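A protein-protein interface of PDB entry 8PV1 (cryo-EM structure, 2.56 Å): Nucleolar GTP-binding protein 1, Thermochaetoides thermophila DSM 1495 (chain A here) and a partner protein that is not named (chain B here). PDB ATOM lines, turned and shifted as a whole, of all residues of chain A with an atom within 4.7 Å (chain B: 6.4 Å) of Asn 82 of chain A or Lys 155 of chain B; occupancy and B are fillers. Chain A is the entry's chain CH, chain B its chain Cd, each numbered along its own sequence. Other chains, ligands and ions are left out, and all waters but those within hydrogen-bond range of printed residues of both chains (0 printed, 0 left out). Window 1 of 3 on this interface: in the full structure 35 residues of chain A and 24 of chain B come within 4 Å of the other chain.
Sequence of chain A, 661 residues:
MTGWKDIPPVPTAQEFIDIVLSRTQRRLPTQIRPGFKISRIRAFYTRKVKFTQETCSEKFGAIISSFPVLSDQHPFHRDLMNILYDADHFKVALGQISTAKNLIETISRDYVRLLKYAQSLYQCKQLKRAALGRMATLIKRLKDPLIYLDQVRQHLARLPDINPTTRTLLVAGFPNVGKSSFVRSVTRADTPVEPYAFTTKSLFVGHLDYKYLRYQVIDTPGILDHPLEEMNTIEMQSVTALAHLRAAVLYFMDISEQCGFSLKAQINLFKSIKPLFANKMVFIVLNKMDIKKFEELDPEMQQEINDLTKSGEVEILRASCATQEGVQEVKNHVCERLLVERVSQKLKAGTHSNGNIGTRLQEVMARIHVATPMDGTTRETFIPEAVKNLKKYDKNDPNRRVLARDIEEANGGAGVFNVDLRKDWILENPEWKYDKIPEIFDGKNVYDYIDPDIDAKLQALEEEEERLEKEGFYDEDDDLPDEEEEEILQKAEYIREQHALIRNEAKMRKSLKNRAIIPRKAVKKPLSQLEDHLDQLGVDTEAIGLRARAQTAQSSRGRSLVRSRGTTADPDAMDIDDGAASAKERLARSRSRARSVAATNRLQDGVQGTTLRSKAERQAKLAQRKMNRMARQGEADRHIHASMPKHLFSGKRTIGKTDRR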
ATOM      1  N   ARG A  78       3.587 -30.321 -15.482  1.00  0.00           N
ATOM      2  CA  ARG A  78       4.751 -30.919 -14.832  1.00  0.00           C
ATOM      3  C   ARG A  78       5.970 -30.012 -14.922  1.00  0.00           C
ATOM      4  O   ARG A  78       6.639 -29.755 -13.911  1.00  0.00           O
ATOM      5  CB  ARG A  78       5.068 -32.274 -15.461  1.00  0.00           C
ATOM      6  CG  ARG A  78       6.185 -33.014 -14.751  1.00  0.00           C
ATOM      7  CD  ARG A  78       6.592 -34.265 -15.498  1.00  0.00           C
ATOM      8  NE  ARG A  78       5.443 -35.010 -15.991  1.00  0.00           N
ATOM      9  CZ  ARG A  78       5.348 -36.331 -15.970  1.00  0.00           C
ATOM     10  NH1 ARG A  78       6.325 -37.087 -15.495  1.00  0.00           N
ATOM     11  NH2 ARG A  78       4.243 -36.909 -16.429  1.00  0.00           N
ATOM     12  N   ASP A  79       6.268 -29.503 -16.118  1.00  0.00           N
ATOM     13  CA  ASP A  79       7.454 -28.670 -16.261  1.00  0.00           C
ATOM     14  C   ASP A  79       7.262 -27.309 -15.603  1.00  0.00           C
ATOM     15  O   ASP A  79       8.220 -26.741 -15.073  1.00  0.00           O
ATOM     16  CB  ASP A  79       7.827 -28.524 -17.732  1.00  0.00           C
ATOM     17  CG  ASP A  79       8.600 -29.713 -18.250  1.00  0.00           C
ATOM     18  OD1 ASP A  79       9.466 -29.524 -19.125  1.00  0.00           O
ATOM     19  OD2 ASP A  79       8.341 -30.841 -17.781  1.00  0.00           O
ATOM     20  N   LEU A  80       6.032 -26.787 -15.597  1.00  0.00           N
ATOM     21  CA  LEU A  80       5.760 -25.536 -14.895  1.00  0.00           C
ATOM     22  C   LEU A  80       5.961 -25.686 -13.393  1.00  0.00           C
ATOM     23  O   LEU A  80       6.540 -24.804 -12.749  1.00  0.00           O
ATOM     24  CB  LEU A  80       4.340 -25.060 -15.193  1.00  0.00           C
ATOM     25  CG  LEU A  80       3.957 -23.722 -14.561  1.00  0.00           C
ATOM     26  CD1 LEU A  80       4.813 -22.598 -15.114  1.00  0.00           C
ATOM     27  CD2 LEU A  80       2.484 -23.432 -14.764  1.00  0.00           C
ATOM     28  N   MET A  81       5.494 -26.797 -12.816  1.00  0.00           N
ATOM     29  CA  MET A  81       5.707 -27.021 -11.390  1.00  0.00           C
ATOM     30  C   MET A  81       7.176 -27.277 -11.084  1.00  0.00           C
ATOM     31  O   MET A  81       7.653 -26.938  -9.996  1.00  0.00           O
ATOM     32  CB  MET A  81       4.836 -28.174 -10.893  1.00  0.00           C
ATOM     33  CG  MET A  81       3.345 -27.877 -10.911  1.00  0.00           C
ATOM     34  SD  MET A  81       2.341 -29.253 -10.328  1.00  0.00           S
ATOM     35  CE  MET A  81       0.695 -28.597 -10.576  1.00  0.00           C
ATOM     36  N   ASN A  82       7.913 -27.871 -12.028  1.00  0.00           N
ATOM     37  CA  ASN A  82       9.355 -28.016 -11.842  1.00  0.00           C
ATOM     38  C   ASN A  82      10.060 -26.663 -11.856  1.00  0.00           C
ATOM     39  O   ASN A  82      11.005 -26.443 -11.090  1.00  0.00           O
ATOM     40  CB  ASN A  82       9.938 -28.931 -12.915  1.00  0.00           C
ATOM     41  CG  ASN A  82      11.453 -28.976 -12.876  1.00  0.00           C
ATOM     42  OD1 ASN A  82      12.050 -29.345 -11.867  1.00  0.00           O
ATOM     43  ND2 ASN A  82      12.084 -28.593 -13.979  1.00  0.00           N
ATOM     44  N   ILE A  83       9.631 -25.754 -12.736  1.00  0.00           N
ATOM     45  CA  ILE A  83      10.207 -24.409 -12.761  1.00  0.00           C
ATOM     46  C   ILE A  83       9.877 -23.662 -11.475  1.00  0.00           C
ATOM     47  O   ILE A  83      10.745 -23.023 -10.869  1.00  0.00           O
ATOM     48  CB  ILE A  83       9.718 -23.632 -14.002  1.00  0.00           C
ATOM     49  CG1 ILE A  83      10.200 -24.290 -15.295  1.00  0.00           C
ATOM     50  CG2 ILE A  83      10.183 -22.187 -13.956  1.00  0.00           C
ATOM     51  CD1 ILE A  83      11.683 -24.437 -15.399  1.00  0.00           C
ATOM     52  N   LEU A  84       8.623 -23.743 -11.029  1.00  0.00           N
ATOM     53  CA  LEU A  84       8.180 -22.940  -9.895  1.00  0.00           C
ATOM     54  C   LEU A  84       8.686 -23.475  -8.559  1.00  0.00           C
ATOM     55  O   LEU A  84       9.106 -22.690  -7.701  1.00  0.00           O
ATOM     56  CB  LEU A  84       6.655 -22.853  -9.876  1.00  0.00           C
ATOM     57  CG  LEU A  84       5.975 -22.054 -10.988  1.00  0.00           C
ATOM     58  CD1 LEU A  84       4.483 -22.330 -10.990  1.00  0.00           C
ATOM     59  CD2 LEU A  84       6.247 -20.572 -10.836  1.00  0.00           C
ATOM     60  N   TYR A  85       8.657 -24.792  -8.349  1.00  0.00           N
ATOM     61  CA  TYR A  85       8.831 -25.339  -7.012  1.00  0.00           C
ATOM     62  C   TYR A  85       9.937 -26.371  -6.861  1.00  0.00           C
ATOM     63  O   TYR A  85      10.042 -26.949  -5.772  1.00  0.00           O
ATOM     64  CB  TYR A  85       7.527 -25.986  -6.522  1.00  0.00           C
ATOM     65  CG  TYR A  85       6.282 -25.196  -6.815  1.00  0.00           C
ATOM     66  CD1 TYR A  85       6.109 -23.921  -6.302  1.00  0.00           C
ATOM     67  CD2 TYR A  85       5.274 -25.732  -7.599  1.00  0.00           C
ATOM     68  CE1 TYR A  85       4.974 -23.200  -6.568  1.00  0.00           C
ATOM     69  CE2 TYR A  85       4.143 -25.014  -7.882  1.00  0.00           C
ATOM     70  CZ  TYR A  85       3.989 -23.754  -7.354  1.00  0.00           C
ATOM     71  OH  TYR A  85       2.847 -23.038  -7.626  1.00  0.00           O
ATOM     72  N   ASP A  86      10.752 -26.623  -7.897  1.00  0.00           N
ATOM     73  CA  ASP A  86      11.825 -27.619  -7.850  1.00  0.00           C
ATOM     74  C   ASP A  86      11.290 -29.016  -7.545  1.00  0.00           C
ATOM     75  O   ASP A  86      11.271 -29.437  -6.379  1.00  0.00           O
ATOM     76  CB  ASP A  86      12.928 -27.227  -6.865  1.00  0.00           C
ATOM     77  CG  ASP A  86      14.142 -28.124  -6.965  1.00  0.00           C
ATOM     78  OD1 ASP A  86      14.350 -28.744  -8.025  1.00  0.00           O
ATOM     79  OD2 ASP A  86      14.899 -28.209  -5.980  1.00  0.00           O
ATOM     80  N   ALA A  87      10.740 -29.661  -8.587  1.00  0.00           N
ATOM     81  CA  ALA A  87      10.149 -31.004  -8.528  1.00  0.00           C
ATOM     82  C   ALA A  87      10.919 -31.982  -7.641  1.00  0.00           C
ATOM     83  O   ALA A  87      10.307 -32.822  -6.970  1.00  0.00           O
ATOM     84  CB  ALA A  87      10.040 -31.569  -9.942  1.00  0.00           C
ATOM     85  N   ASP A  88      12.254 -31.907  -7.637  1.00  0.00           N
ATOM     86  CA  ASP A  88      13.046 -32.723  -6.719  1.00  0.00           C
ATOM     87  C   ASP A  88      12.692 -32.431  -5.264  1.00  0.00           C
ATOM     88  O   ASP A  88      12.394 -33.351  -4.494  1.00  0.00           O
ATOM     89  CB  ASP A  88      14.537 -32.493  -6.962  1.00  0.00           C
ATOM     90  CG  ASP A  88      15.055 -33.255  -8.159  1.00  0.00           C
ATOM     91  OD1 ASP A  88      14.450 -34.286  -8.517  1.00  0.00           O
ATOM     92  OD2 ASP A  88      16.072 -32.827  -8.740  1.00  0.00           O
ATOM     93  N   ARG B 138      22.626 -29.980  -0.256  1.00  0.00           N
ATOM     94  CA  ARG B 138      23.140 -29.063  -1.269  1.00  0.00           C
ATOM     95  C   ARG B 138      22.363 -27.755  -1.287  1.00  0.00           C
ATOM     96  O   ARG B 138      22.957 -26.676  -1.373  1.00  0.00           O
ATOM     97  CB  ARG B 138      23.099 -29.724  -2.643  1.00  0.00           C
ATOM     98  CG  ARG B 138      23.660 -28.860  -3.754  1.00  0.00           C
ATOM     99  CD  ARG B 138      23.230 -29.339  -5.132  1.00  0.00           C
ATOM    100  NE  ARG B 138      23.258 -30.792  -5.258  1.00  0.00           N
ATOM    101  CZ  ARG B 138      22.187 -31.552  -5.431  1.00  0.00           C
ATOM    102  NH1 ARG B 138      20.974 -31.030  -5.509  1.00  0.00           N
ATOM    103  NH2 ARG B 138      22.333 -32.870  -5.525  1.00  0.00           N
ATOM    104  N   GLU B 139      21.037 -27.826  -1.213  1.00  0.00           N
ATOM    105  CA  GLU B 139      20.198 -26.629  -1.212  1.00  0.00           C
ATOM    106  C   GLU B 139      18.943 -26.853  -0.370  1.00  0.00           C
ATOM    107  O   GLU B 139      18.143 -27.763  -0.651  1.00  0.00           O
ATOM    108  CB  GLU B 139      19.916 -26.182  -2.648  1.00  0.00           C
ATOM    109  CG  GLU B 139      19.105 -27.112  -3.531  1.00  0.00           C
ATOM    110  CD  GLU B 139      18.949 -26.594  -4.948  1.00  0.00           C
ATOM    111  OE1 GLU B 139      19.495 -25.513  -5.253  1.00  0.00           O
ATOM    112  OE2 GLU B 139      18.288 -27.274  -5.763  1.00  0.00           O
ATOM    113  N   ARG B 151      16.836 -19.222  -5.030  1.00  0.00           N
ATOM    114  CA  ARG B 151      16.956 -20.019  -6.242  1.00  0.00           C
ATOM    115  C   ARG B 151      16.574 -19.192  -7.463  1.00  0.00           C
ATOM    116  O   ARG B 151      15.506 -18.574  -7.499  1.00  0.00           O
ATOM    117  CB  ARG B 151      16.068 -21.256  -6.133  1.00  0.00           C
ATOM    118  CG  ARG B 151      15.830 -21.999  -7.431  1.00  0.00           C
ATOM    119  CD  ARG B 151      14.969 -23.220  -7.177  1.00  0.00           C
ATOM    120  NE  ARG B 151      14.665 -23.965  -8.391  1.00  0.00           N
ATOM    121  CZ  ARG B 151      13.553 -23.823  -9.098  1.00  0.00           C
ATOM    122  NH1 ARG B 151      12.622 -22.948  -8.755  1.00  0.00           N
ATOM    123  NH2 ARG B 151      13.369 -24.579 -10.176  1.00  0.00           N
ATOM    124  N   ARG B 153      18.137 -20.235 -11.057  1.00  0.00           N
ATOM    125  CA  ARG B 153      18.130 -21.132 -12.205  1.00  0.00           C
ATOM    126  C   ARG B 153      17.460 -22.445 -11.845  1.00  0.00           C
ATOM    127  O   ARG B 153      17.726 -22.996 -10.768  1.00  0.00           O
ATOM    128  CB  ARG B 153      19.548 -21.402 -12.701  1.00  0.00           C
ATOM    129  CG  ARG B 153      20.121 -20.338 -13.623  1.00  0.00           C
ATOM    130  CD  ARG B 153      20.808 -19.223 -12.867  1.00  0.00           C
ATOM    131  NE  ARG B 153      21.563 -18.364 -13.770  1.00  0.00           N
ATOM    132  CZ  ARG B 153      21.097 -17.247 -14.309  1.00  0.00           C
ATOM    133  NH1 ARG B 153      19.875 -16.811 -14.049  1.00  0.00           N
ATOM    134  NH2 ARG B 153      21.876 -16.549 -15.129  1.00  0.00           N
ATOM    135  N   PRO B 154      16.596 -22.971 -12.704  1.00  0.00           N
ATOM    136  CA  PRO B 154      15.990 -24.278 -12.449  1.00  0.00           C
ATOM    137  C   PRO B 154      16.922 -25.410 -12.864  1.00  0.00           C
ATOM    138  O   PRO B 154      17.967 -25.205 -13.480  1.00  0.00           O
ATOM    139  CB  PRO B 154      14.733 -24.250 -13.318  1.00  0.00           C
ATOM    140  CG  PRO B 154      15.119 -23.384 -14.467  1.00  0.00           C
ATOM    141  CD  PRO B 154      16.062 -22.344 -13.925  1.00  0.00           C
ATOM    142  N   LYS B 155      16.517 -26.624 -12.509  1.00  0.00           N
ATOM    143  CA  LYS B 155      17.224 -27.833 -12.909  1.00  0.00           C
ATOM    144  C   LYS B 155      16.507 -28.439 -14.108  1.00  0.00           C
ATOM    145  O   LYS B 155      15.335 -28.813 -14.012  1.00  0.00           O
ATOM    146  CB  LYS B 155      17.293 -28.835 -11.758  1.00  0.00           C
ATOM    147  CG  LYS B 155      18.053 -30.103 -12.094  1.00  0.00           C
ATOM    148  CD  LYS B 155      18.094 -31.047 -10.910  1.00  0.00           C
ATOM    149  CE  LYS B 155      18.883 -32.301 -11.239  1.00  0.00           C
ATOM    150  NZ  LYS B 155      18.204 -33.115 -12.282  1.00  0.00           N
ATOM    151  N   LEU B 156      17.211 -28.535 -15.231  1.00  0.00           N
ATOM    152  CA  LEU B 156      16.626 -28.980 -16.484  1.00  0.00           C
ATOM    153  C   LEU B 156      17.327 -30.239 -16.978  1.00  0.00           C
ATOM    154  O   LEU B 156      18.521 -30.446 -16.744  1.00  0.00           O
ATOM    155  CB  LEU B 156      16.712 -27.884 -17.552  1.00  0.00           C
ATOM    156  CG  LEU B 156      16.206 -26.506 -17.127  1.00  0.00           C
ATOM    157  CD1 LEU B 156      16.559 -25.459 -18.166  1.00  0.00           C
ATOM    158  CD2 LEU B 156      14.712 -26.543 -16.880  1.00  0.00           C
ATOM    159  N   SER B 157      16.562 -31.083 -17.666  1.00  0.00           N
ATOM    160  CA  SER B 157      17.082 -32.288 -18.292  1.00  0.00           C
ATOM    161  C   SER B 157      17.492 -32.054 -19.739  1.00  0.00           C
ATOM    162  O   SER B 157      17.843 -33.009 -20.438  1.00  0.00           O
ATOM    163  CB  SER B 157      16.045 -33.410 -18.219  1.00  0.00           C
ATOM    164  OG  SER B 157      14.796 -32.978 -18.730  1.00  0.00           O
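NH2 of Arg 151 of chain B is in hydrogen-bond range of O of Asn 82 of chain A, 3.1 Å away. The guanidinium group (NH1) of Arg 151 of chain B lies within hydrogen-bond range of the backbone carbonyl oxygen (O) of Ile 83 of chain A (2.8 Å). ND2 of Asn 82 of chain A sits at hydrogen-bond distance from O of Lys 155 of chain B, 3.3 Å away.
Of the 8 printed residues of chain B, 5 touch a printed residue of chain A. Printed residues of chain B that touch a printed residue of chain A: Glu 139, Arg 151, Pro 154, Lys 155 and Leu 156. Among the printed residues, no Asp or Glu carboxylate lies within 4 Å of a Lys or Arg side-chain nitrogen of the other chain.
Among the printed residues, pairs that only touch across the chains: Ile 83 of chain A with Pro 154 of chain B, Ile 83 of chain A with Leu 156 of chain B, Leu 84 of chain A with Arg 151 of chain B, Asp 86 of chain A with Glu 139 of chain B, Asp 86 of chain A with Arg 151 of chain B and Asp 88 of chain A with Lys 155 of chain B.
Printed residues of chain B within 4 Å of Asn 82 of chain A: Arg 151 and Lys 155. Of the printed residues of chain B, Ile 83 of chain A touches Arg 151, Pro 154 and Leu 156. Of the printed residues of chain A, Pro 154 of chain B touches Ile 83 (3.7 Å). The nearest residue of chain B that does not touch Asn 82 of chain A is Leu 156 of chain B (4.4 Å). The nearest printed residue of chain A that does not touch Lys 155 of chain B is Asp 86 of chain A (4.8 Å).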
